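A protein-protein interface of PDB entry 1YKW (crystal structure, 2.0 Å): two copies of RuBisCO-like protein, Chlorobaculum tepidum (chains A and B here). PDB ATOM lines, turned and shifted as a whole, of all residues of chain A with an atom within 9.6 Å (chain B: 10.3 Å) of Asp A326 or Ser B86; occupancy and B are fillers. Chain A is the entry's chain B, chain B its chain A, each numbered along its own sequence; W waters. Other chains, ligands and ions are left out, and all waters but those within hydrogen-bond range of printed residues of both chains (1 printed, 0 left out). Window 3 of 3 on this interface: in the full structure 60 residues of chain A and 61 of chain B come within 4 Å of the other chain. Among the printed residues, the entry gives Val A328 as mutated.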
ATOM      1  N   GLY A 323      10.414  16.664 -22.760  1.00  0.00           N
ATOM      2  CA  GLY A 323      10.698  17.044 -21.395  1.00  0.00           C
ATOM      3  C   GLY A 323      10.979  15.906 -20.441  1.00  0.00           C
ATOM      4  O   GLY A 323      11.493  14.845 -20.827  1.00  0.00           O
ATOM      5  N   PHE A 324      10.642  16.154 -19.175  1.00  0.00           N
ATOM      6  CA  PHE A 324      10.799  15.169 -18.103  1.00  0.00           C
ATOM      7  C   PHE A 324       9.577  14.278 -17.907  1.00  0.00           C
ATOM      8  O   PHE A 324       8.455  14.640 -18.269  1.00  0.00           O
ATOM      9  CB  PHE A 324      11.163  15.885 -16.792  1.00  0.00           C
ATOM     10  CG  PHE A 324      12.269  16.887 -16.941  1.00  0.00           C
ATOM     11  CD1 PHE A 324      11.971  18.251 -17.028  1.00  0.00           C
ATOM     12  CD2 PHE A 324      13.602  16.478 -17.037  1.00  0.00           C
ATOM     13  CE1 PHE A 324      12.955  19.193 -17.154  1.00  0.00           C
ATOM     14  CE2 PHE A 324      14.617  17.424 -17.161  1.00  0.00           C
ATOM     15  CZ  PHE A 324      14.287  18.801 -17.237  1.00  0.00           C
ATOM     16  N   GLY A 325       9.813  13.093 -17.349  1.00  0.00           N
ATOM     17  CA  GLY A 325       8.752  12.114 -17.096  1.00  0.00           C
ATOM     18  C   GLY A 325       9.115  10.731 -17.597  1.00  0.00           C
ATOM     19  O   GLY A 325       9.746  10.587 -18.643  1.00  0.00           O
ATOM     20  N   ASP A 326       8.733   9.694 -16.861  1.00  0.00           N
ATOM     21  CA  ASP A 326       9.217   8.362 -17.229  1.00  0.00           C
ATOM     22  C   ASP A 326       8.650   7.888 -18.567  1.00  0.00           C
ATOM     23  O   ASP A 326       9.242   7.031 -19.236  1.00  0.00           O
ATOM     24  CB  ASP A 326       9.031   7.343 -16.092  1.00  0.00           C
ATOM     25  CG  ASP A 326       7.579   6.914 -15.893  1.00  0.00           C
ATOM     26  OD1 ASP A 326       6.663   7.724 -16.183  1.00  0.00           O
ATOM     27  OD2 ASP A 326       7.370   5.758 -15.426  1.00  0.00           O
ATOM     28  N   ARG A 327       7.517   8.458 -18.975  1.00  0.00           N
ATOM     29  CA  ARG A 327       6.964   8.111 -20.292  1.00  0.00           C
ATOM     30  C   ARG A 327       7.526   8.907 -21.492  1.00  0.00           C
ATOM     31  O   ARG A 327       7.141   8.648 -22.636  1.00  0.00           O
ATOM     32  CB  ARG A 327       5.427   8.082 -20.284  1.00  0.00           C
ATOM     33  CG  ARG A 327       4.738   9.409 -19.978  1.00  0.00           C
ATOM     34  CD  ARG A 327       3.226   9.303 -20.191  1.00  0.00           C
ATOM     35  NE  ARG A 327       2.551   8.469 -19.189  1.00  0.00           N
ATOM     36  CZ  ARG A 327       1.817   8.939 -18.178  1.00  0.00           C
ATOM     37  NH1 ARG A 327       1.648  10.248 -18.007  1.00  0.00           N
ATOM     38  NH2 ARG A 327       1.245   8.091 -17.328  1.00  0.00           N
ATOM     39  N   VAL A 328       8.440   9.845 -21.241  1.00  0.00           N
ATOM     40  CA  VAL A 328       9.105  10.581 -22.333  1.00  0.00           C
ATOM     41  C   VAL A 328      10.303   9.751 -22.808  1.00  0.00           C
ATOM     42  O   VAL A 328      11.073   9.222 -21.993  1.00  0.00           O
ATOM     43  CB  VAL A 328       9.583  11.992 -21.926  1.00  0.00           C
ATOM     44  CG1 VAL A 328       9.937  12.814 -23.148  1.00  0.00           C
ATOM     45  CG2 VAL A 328       8.520  12.731 -21.101  1.00  0.00           C
ATOM     46  N   MET A 329      10.458   9.630 -24.120  1.00  0.00           N
ATOM     47  CA  MET A 329      11.439   8.696 -24.677  1.00  0.00           C
ATOM     48  C   MET A 329      12.807   9.313 -24.992  1.00  0.00           C
ATOM     49  O   MET A 329      13.489   8.914 -25.944  1.00  0.00           O
ATOM     50  CB  MET A 329      10.838   7.933 -25.864  1.00  0.00           C
ATOM     51  CG  MET A 329       9.813   6.873 -25.431  1.00  0.00           C
ATOM     52  SD  MET A 329       9.250   5.736 -26.722  1.00  0.00           S
ATOM     53  CE  MET A 329       7.992   6.724 -27.511  1.00  0.00           C
ATOM     54  N   THR A 330      13.182  10.295 -24.177  1.00  0.00           N
ATOM     55  CA  THR A 330      14.483  10.934 -24.194  1.00  0.00           C
ATOM     56  C   THR A 330      15.011  10.901 -22.756  1.00  0.00           C
ATOM     57  O   THR A 330      14.285  11.285 -21.841  1.00  0.00           O
ATOM     58  CB  THR A 330      14.377  12.424 -24.635  1.00  0.00           C
ATOM     59  OG1 THR A 330      13.796  12.508 -25.950  1.00  0.00           O
ATOM     60  CG2 THR A 330      15.744  13.070 -24.643  1.00  0.00           C
ATOM     61  N   PRO A 331      16.272  10.450 -22.545  1.00  0.00           N
ATOM     62  CA  PRO A 331      16.849  10.459 -21.186  1.00  0.00           C
ATOM     63  C   PRO A 331      16.818  11.843 -20.530  1.00  0.00           C
ATOM     64  O   PRO A 331      16.980  12.864 -21.209  1.00  0.00           O
ATOM     65  CB  PRO A 331      18.307  10.059 -21.427  1.00  0.00           C
ATOM     66  CG  PRO A 331      18.318   9.331 -22.695  1.00  0.00           C
ATOM     67  CD  PRO A 331      17.229   9.932 -23.546  1.00  0.00           C
ATOM     68  N   GLU A 332      16.626  11.875 -19.219  1.00  0.00           N
ATOM     69  CA  GLU A 332      16.561  13.120 -18.453  1.00  0.00           C
ATOM     70  C   GLU A 332      17.807  14.009 -18.616  1.00  0.00           C
ATOM     71  O   GLU A 332      17.678  15.223 -18.753  1.00  0.00           O
ATOM     72  CB  GLU A 332      16.317  12.808 -16.972  1.00  0.00           C
ATOM     73  CG  GLU A 332      16.264  14.008 -16.040  1.00  0.00           C
ATOM     74  CD  GLU A 332      15.963  13.598 -14.604  1.00  0.00           C
ATOM     75  OE1 GLU A 332      15.048  12.769 -14.413  1.00  0.00           O
ATOM     76  OE2 GLU A 332      16.627  14.108 -13.669  1.00  0.00           O
ATOM     77  N   GLY A 358       6.661  17.444 -21.214  1.00  0.00           N
ATOM     78  CA  GLY A 358       6.629  16.040 -20.797  1.00  0.00           C
ATOM     79  C   GLY A 358       5.230  15.597 -20.413  1.00  0.00           C
ATOM     80  O   GLY A 358       4.230  16.114 -20.917  1.00  0.00           O
ATOM     81  N   SER A 359       5.169  14.642 -19.493  1.00  0.00           N
ATOM     82  CA  SER A 359       3.899  14.198 -18.948  1.00  0.00           C
ATOM     83  C   SER A 359       3.460  15.152 -17.835  1.00  0.00           C
ATOM     84  O   SER A 359       3.288  14.741 -16.690  1.00  0.00           O
ATOM     85  CB  SER A 359       3.996  12.748 -18.452  1.00  0.00           C
ATOM     86  OG  SER A 359       5.348  12.333 -18.270  1.00  0.00           O
ATOM     87  N   ASP A 360       3.249  16.415 -18.191  1.00  0.00           N
ATOM     88  CA  ASP A 360       3.135  17.478 -17.202  1.00  0.00           C
ATOM     89  C   ASP A 360       1.702  17.834 -16.801  1.00  0.00           C
ATOM     90  O   ASP A 360       0.782  17.704 -17.610  1.00  0.00           O
ATOM     91  CB  ASP A 360       3.886  18.728 -17.663  1.00  0.00           C
ATOM     92  CG  ASP A 360       5.416  18.546 -17.656  1.00  0.00           C
ATOM     93  OD1 ASP A 360       5.954  17.882 -16.735  1.00  0.00           O
ATOM     94  OD2 ASP A 360       6.089  19.079 -18.568  1.00  0.00           O
ATOM     95  N   THR A 364       3.186  18.191 -11.522  1.00  0.00           N
ATOM     96  CA  THR A 364       4.590  17.962 -11.884  1.00  0.00           C
ATOM     97  C   THR A 364       5.401  19.256 -11.988  1.00  0.00           C
ATOM     98  O   THR A 364       6.606  19.236 -12.285  1.00  0.00           O
ATOM     99  CB  THR A 364       4.725  17.260 -13.234  1.00  0.00           C
ATOM    100  OG1 THR A 364       4.183  18.112 -14.249  1.00  0.00           O
ATOM    101  CG2 THR A 364       4.038  15.898 -13.253  1.00  0.00           C
ATOM    102  N   THR A 367       8.609  19.598  -9.698  1.00  0.00           N
ATOM    103  CA  THR A 367       9.695  18.716 -10.198  1.00  0.00           C
ATOM    104  C   THR A 367      10.474  19.333 -11.350  1.00  0.00           C
ATOM    105  O   THR A 367      11.710  19.227 -11.428  1.00  0.00           O
ATOM    106  CB  THR A 367       9.119  17.348 -10.660  1.00  0.00           C
ATOM    107  OG1 THR A 367       8.423  16.752  -9.565  1.00  0.00           O
ATOM    108  CG2 THR A 367      10.222  16.421 -11.131  1.00  0.00           C
ATOM    109  N   LYS A 371      14.339  20.586 -11.417  1.00  0.00           N
ATOM    110  CA  LYS A 371      15.299  20.019 -12.377  1.00  0.00           C
ATOM    111  C   LYS A 371      15.985  21.115 -13.163  1.00  0.00           C
ATOM    112  O   LYS A 371      17.176  21.042 -13.443  1.00  0.00           O
ATOM    113  CB  LYS A 371      14.611  19.062 -13.370  1.00  0.00           C
ATOM    114  CG  LYS A 371      14.019  17.799 -12.724  1.00  0.00           C
ATOM    115  CD  LYS A 371      15.019  16.662 -12.704  1.00  0.00           C
ATOM    116  CE  LYS A 371      14.712  15.646 -11.599  1.00  0.00           C
ATOM    117  NZ  LYS A 371      13.469  14.891 -11.889  1.00  0.00           N
ATOM    118  N   ARG A 383      -1.962  17.211 -19.656  1.00  0.00           N
ATOM    119  CA  ARG A 383      -3.315  16.884 -19.213  1.00  0.00           C
ATOM    120  C   ARG A 383      -3.674  17.721 -17.989  1.00  0.00           C
ATOM    121  O   ARG A 383      -2.800  18.303 -17.343  1.00  0.00           O
ATOM    122  CB  ARG A 383      -3.476  15.391 -18.873  1.00  0.00           C
ATOM    123  CG  ARG A 383      -2.900  14.373 -19.878  1.00  0.00           C
ATOM    124  CD  ARG A 383      -1.392  14.124 -19.656  1.00  0.00           C
ATOM    125  NE  ARG A 383      -1.000  14.327 -18.257  1.00  0.00           N
ATOM    126  CZ  ARG A 383      -1.046  13.390 -17.313  1.00  0.00           C
ATOM    127  NH1 ARG A 383      -1.451  12.163 -17.616  1.00  0.00           N
ATOM    128  NH2 ARG A 383      -0.682  13.677 -16.068  1.00  0.00           N
ATOM    129  N   VAL B  31       5.037  -2.507 -27.774  1.00  0.00           N
ATOM    130  CA  VAL B  31       5.096  -3.060 -26.427  1.00  0.00           C
ATOM    131  C   VAL B  31       3.668  -3.162 -25.874  1.00  0.00           C
ATOM    132  O   VAL B  31       2.908  -2.181 -25.868  1.00  0.00           O
ATOM    133  CB  VAL B  31       5.967  -2.168 -25.497  1.00  0.00           C
ATOM    134  CG1 VAL B  31       6.036  -2.750 -24.103  1.00  0.00           C
ATOM    135  CG2 VAL B  31       7.381  -1.956 -26.072  1.00  0.00           C
ATOM    136  N   GLY B  32       3.288  -4.351 -25.418  1.00  0.00           N
ATOM    137  CA  GLY B  32       1.933  -4.580 -24.941  1.00  0.00           C
ATOM    138  C   GLY B  32       1.054  -5.048 -26.079  1.00  0.00           C
ATOM    139  O   GLY B  32       1.555  -5.515 -27.104  1.00  0.00           O
ATOM    140  N   LEU B  79      13.957  -4.956 -27.492  1.00  0.00           N
ATOM    141  CA  LEU B  79      13.943  -4.014 -28.602  1.00  0.00           C
ATOM    142  C   LEU B  79      15.256  -4.117 -29.384  1.00  0.00           C
ATOM    143  O   LEU B  79      16.274  -4.526 -28.824  1.00  0.00           O
ATOM    144  CB  LEU B  79      13.756  -2.591 -28.061  1.00  0.00           C
ATOM    145  CG  LEU B  79      12.451  -1.773 -28.026  1.00  0.00           C
ATOM    146  CD1 LEU B  79      11.132  -2.536 -28.042  1.00  0.00           C
ATOM    147  CD2 LEU B  79      12.486  -0.788 -26.858  1.00  0.00           C
ATOM    148  N   PRO B  82      18.269  -0.051 -27.583  1.00  0.00           N
ATOM    149  CA  PRO B  82      17.822   0.186 -26.193  1.00  0.00           C
ATOM    150  C   PRO B  82      17.254   1.593 -25.906  1.00  0.00           C
ATOM    151  O   PRO B  82      17.901   2.384 -25.224  1.00  0.00           O
ATOM    152  CB  PRO B  82      19.108  -0.009 -25.392  1.00  0.00           C
ATOM    153  CG  PRO B  82      20.181   0.485 -26.322  1.00  0.00           C
ATOM    154  CD  PRO B  82      19.732   0.091 -27.720  1.00  0.00           C
ATOM    155  N   VAL B  83      16.049   1.892 -26.382  1.00  0.00           N
ATOM    156  CA  VAL B  83      15.401   3.200 -26.167  1.00  0.00           C
ATOM    157  C   VAL B  83      14.846   3.329 -24.744  1.00  0.00           C
ATOM    158  O   VAL B  83      14.269   2.369 -24.193  1.00  0.00           O
ATOM    159  CB  VAL B  83      14.262   3.391 -27.179  1.00  0.00           C
ATOM    160  CG1 VAL B  83      13.625   4.799 -27.089  1.00  0.00           C
ATOM    161  CG2 VAL B  83      14.790   3.118 -28.564  1.00  0.00           C
ATOM    162  N   LYS B  84      15.031   4.509 -24.151  1.00  0.00           N
ATOM    163  CA  LYS B  84      14.416   4.834 -22.868  1.00  0.00           C
ATOM    164  C   LYS B  84      12.891   4.755 -22.965  1.00  0.00           C
ATOM    165  O   LYS B  84      12.285   5.489 -23.740  1.00  0.00           O
ATOM    166  CB  LYS B  84      14.832   6.232 -22.410  1.00  0.00           C
ATOM    167  CG  LYS B  84      14.435   6.529 -20.971  1.00  0.00           C
ATOM    168  CD  LYS B  84      13.889   7.942 -20.844  1.00  0.00           C
ATOM    169  CE  LYS B  84      13.398   8.223 -19.452  1.00  0.00           C
ATOM    170  NZ  LYS B  84      12.137   8.982 -19.523  1.00  0.00           N
ATOM    171  N   HIS B  85      12.279   3.840 -22.214  1.00  0.00           N
ATOM    172  CA  HIS B  85      10.816   3.706 -22.214  1.00  0.00           C
ATOM    173  C   HIS B  85      10.279   3.073 -20.924  1.00  0.00           C
ATOM    174  O   HIS B  85      10.931   2.199 -20.318  1.00  0.00           O
ATOM    175  CB  HIS B  85      10.328   2.959 -23.466  1.00  0.00           C
ATOM    176  CG  HIS B  85      10.629   1.493 -23.452  1.00  0.00           C
ATOM    177  ND1 HIS B  85      11.908   0.995 -23.572  1.00  0.00           N
ATOM    178  CD2 HIS B  85       9.815   0.419 -23.327  1.00  0.00           C
ATOM    179  CE1 HIS B  85      11.871  -0.323 -23.512  1.00  0.00           C
ATOM    180  NE2 HIS B  85      10.613  -0.698 -23.362  1.00  0.00           N
ATOM    181  N   SER B  86       9.096   3.523 -20.510  1.00  0.00           N
ATOM    182  CA  SER B  86       8.474   3.064 -19.265  1.00  0.00           C
ATOM    183  C   SER B  86       7.571   1.857 -19.498  1.00  0.00           C
ATOM    184  O   SER B  86       7.376   1.045 -18.586  1.00  0.00           O
ATOM    185  CB  SER B  86       7.671   4.188 -18.596  1.00  0.00           C
ATOM    186  OG  SER B  86       6.797   4.801 -19.538  1.00  0.00           O
ATOM    187  N   GLU B  87       7.039   1.733 -20.714  1.00  0.00           N
ATOM    188  CA  GLU B  87       6.060   0.686 -21.031  1.00  0.00           C
ATOM    189  C   GLU B  87       6.611  -0.710 -20.765  1.00  0.00           C
ATOM    190  O   GLU B  87       7.791  -0.992 -20.989  1.00  0.00           O
ATOM    191  CB  GLU B  87       5.541   0.776 -22.477  1.00  0.00           C
ATOM    192  CG  GLU B  87       5.451   2.188 -23.064  1.00  0.00           C
ATOM    193  CD  GLU B  87       4.357   3.049 -22.438  1.00  0.00           C
ATOM    194  OE1 GLU B  87       3.325   2.498 -21.989  1.00  0.00           O
ATOM    195  OE2 GLU B  87       4.528   4.290 -22.401  1.00  0.00           O
ATOM    196  N   THR B  88       5.740  -1.574 -20.263  1.00  0.00           N
ATOM    197  CA  THR B  88       6.087  -2.964 -20.051  1.00  0.00           C
ATOM    198  C   THR B  88       5.143  -3.864 -20.859  1.00  0.00           C
ATOM    199  O   THR B  88       4.048  -3.454 -21.273  1.00  0.00           O
ATOM    200  CB  THR B  88       6.151  -3.324 -18.543  1.00  0.00           C
ATOM    201  OG1 THR B  88       5.027  -2.761 -17.848  1.00  0.00           O
ATOM    202  CG2 THR B  88       7.435  -2.774 -17.916  1.00  0.00           C
ATOM    203  N   GLY B  89       5.601  -5.077 -21.139  1.00  0.00           N
ATOM    204  CA  GLY B  89       4.793  -6.015 -21.903  1.00  0.00           C
ATOM    205  C   GLY B  89       5.566  -6.714 -22.996  1.00  0.00           C
ATOM    206  O   GLY B  89       6.737  -6.413 -23.224  1.00  0.00           O
ATOM    207  N   ILE B  91       7.046  -7.706 -26.463  1.00  0.00           N
ATOM    208  CA  ILE B  91       7.633  -6.949 -27.558  1.00  0.00           C
ATOM    209  C   ILE B  91       7.426  -7.723 -28.861  1.00  0.00           C
ATOM    210  O   ILE B  91       7.752  -8.907 -28.936  1.00  0.00           O
ATOM    211  CB  ILE B  91       9.147  -6.652 -27.313  1.00  0.00           C
ATOM    212  CG1 ILE B  91       9.359  -5.858 -26.007  1.00  0.00           C
ATOM    213  CG2 ILE B  91       9.703  -5.815 -28.447  1.00  0.00           C
ATOM    214  CD1 ILE B  91      10.790  -5.924 -25.448  1.00  0.00           C
ATOM    215  N   PHE B 123       7.177   9.309 -30.975  1.00  0.00           N
ATOM    216  CA  PHE B 123       6.904   9.449 -29.560  1.00  0.00           C
ATOM    217  C   PHE B 123       5.554   8.862 -29.124  1.00  0.00           C
ATOM    218  O   PHE B 123       5.004   9.317 -28.132  1.00  0.00           O
ATOM    219  CB  PHE B 123       6.995  10.920 -29.139  1.00  0.00           C
ATOM    220  CG  PHE B 123       8.391  11.500 -29.187  1.00  0.00           C
ATOM    221  CD1 PHE B 123       8.815  12.226 -30.299  1.00  0.00           C
ATOM    222  CD2 PHE B 123       9.259  11.337 -28.108  1.00  0.00           C
ATOM    223  CE1 PHE B 123      10.100  12.774 -30.336  1.00  0.00           C
ATOM    224  CE2 PHE B 123      10.549  11.900 -28.124  1.00  0.00           C
ATOM    225  CZ  PHE B 123      10.963  12.610 -29.236  1.00  0.00           C
ATOM    226  N   THR B 124       5.018   7.869 -29.845  1.00  0.00           N
ATOM    227  CA  THR B 124       3.830   7.132 -29.337  1.00  0.00           C
ATOM    228  C   THR B 124       4.261   6.193 -28.202  1.00  0.00           C
ATOM    229  O   THR B 124       5.178   5.384 -28.377  1.00  0.00           O
ATOM    230  CB  THR B 124       3.104   6.300 -30.450  1.00  0.00           C
ATOM    231  OG1 THR B 124       2.669   7.162 -31.508  1.00  0.00           O
ATOM    232  CG2 THR B 124       1.897   5.514 -29.915  1.00  0.00           C
ATOM    233  N   PRO B 125       3.586   6.267 -27.042  1.00  0.00           N
ATOM    234  CA  PRO B 125       3.913   5.371 -25.940  1.00  0.00           C
ATOM    235  C   PRO B 125       3.617   3.918 -26.347  1.00  0.00           C
ATOM    236  O   PRO B 125       2.518   3.618 -26.857  1.00  0.00           O
ATOM    237  CB  PRO B 125       2.976   5.836 -24.813  1.00  0.00           C
ATOM    238  CG  PRO B 125       2.610   7.278 -25.201  1.00  0.00           C
ATOM    239  CD  PRO B 125       2.515   7.218 -26.688  1.00  0.00           C
ATOM    240  N   GLY B 126       4.605   3.043 -26.144  1.00  0.00           N
ATOM    241  CA  GLY B 126       4.460   1.632 -26.496  1.00  0.00           C
ATOM    242  C   GLY B 126       4.982   1.305 -27.876  1.00  0.00           C
ATOM    243  O   GLY B 126       4.897   0.163 -28.322  1.00  0.00           O
ATOM    244  N   VAL B 127       5.490   2.306 -28.582  1.00  0.00           N
ATOM    245  CA  VAL B 127       6.095   2.082 -29.898  1.00  0.00           C
ATOM    246  C   VAL B 127       7.424   2.836 -29.959  1.00  0.00           C
ATOM    247  O   VAL B 127       7.496   3.912 -30.542  1.00  0.00           O
ATOM    248  CB  VAL B 127       5.163   2.508 -31.059  1.00  0.00           C
ATOM    249  CG1 VAL B 127       5.604   1.820 -32.329  1.00  0.00           C
ATOM    250  CG2 VAL B 127       3.698   2.143 -30.784  1.00  0.00           C
ATOM    251  N   PRO B 128       8.463   2.295 -29.303  1.00  0.00           N
ATOM    252  CA  PRO B 128       9.741   3.016 -29.197  1.00  0.00           C
ATOM    253  C   PRO B 128      10.669   2.974 -30.428  1.00  0.00           C
ATOM    254  O   PRO B 128      11.581   3.792 -30.548  1.00  0.00           O
ATOM    255  CB  PRO B 128      10.428   2.354 -28.003  1.00  0.00           C
ATOM    256  CG  PRO B 128       9.524   1.184 -27.574  1.00  0.00           C
ATOM    257  CD  PRO B 128       8.492   0.993 -28.615  1.00  0.00           C
HETATM  258  O   HOH W   1       8.093   5.591 -21.990  1.00  0.00           O
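The side-chain amino group (NZ) of Lys B84 lies within hydrogen-bond range of the backbone carbonyl oxygen (O) of Gly A325 (3.0 Å).
The backbone carbonyl oxygen (O) of Asp A326 lies close to the side-chain hydroxyl (OG) of Ser B86, at 3.3 Å.
The backbone carbonyl oxygen of Val A328 is in hydrogen-bond range of the side-chain amino group of Lys B84 (2.7 Å).
Among the printed residues, merely in contact across the chains: Met A329 with Thr B124 (3.2 Å), Met A329 with Lys B84 (3.3 Å), Arg A327 with Ser B86 (3.4 Å), Asp A326 with Lys B84 (3.5 Å), Thr A330 with Lys B84 (3.5 Å), Met A329 with Phe B123 (3.6 Å), Met A329 with Pro B128 (3.7 Å), Pro A331 with Lys B84 (3.9 Å) and Thr A330 with Phe B123 (3.95 Å).
Of the printed residues of chain A, Ser B86 touches Asp A326 (3.3 Å) and Arg A327 (3.4 Å).
Glu B87 touches none of the printed residues of chain A.
Of the printed residues of chain B, Thr A330 touches Lys B84 (3.5 Å) and Phe B123 (3.95 Å).
Of the printed residues of chain B, Pro A331 touches Lys B84 (3.9 Å).
Of the printed residues of chain A, Thr B124 touches Met A329.
Printed residues of chain B within 4 Å of Val A328: Lys B84.
Of the printed residues of chain B, Met A329 touches Lys B84, Phe B123, Thr B124 and Pro B128.
Arg A383 touches none of the printed residues of chain B.
The nearest residue of chain B that does not touch Asp A326 is His B85 (4.4 Å).
The nearest printed residue of chain A that does not touch Thr B124 is Arg A327 (6.7 Å).
Of the 17 printed residues of chain A, 7 touch a printed residue of chain B.
Printed residues of chain A that touch a printed residue of chain B: Gly A325, Asp A326, Arg A327, Val A328, Met A329, Thr A330 and Pro A331.
Hydrophobic or aromatic side chains of chain A that line the printed part of chain B: Met A329.
Along chain A the printed residues that touch a printed residue of chain B span positions 325 to 331.
Of the 18 printed residues of chain B, 5 touch a printed residue of chain A.
Along chain B the printed residues that touch a printed residue of chain A span positions 84 to 128.
Among the printed residues, 12 pairs touch across the chains.
No position is printed for both chains.
Of the 12 pairs that touch across the chains among the printed residues, none has its exchanged pair printed and touching as well.
Water W1 lies within hydrogen-bond range of N of Ser B86 (2.7 Å), O of Arg A327 (3.3 Å) and O of Asp A326 (3.3 Å).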
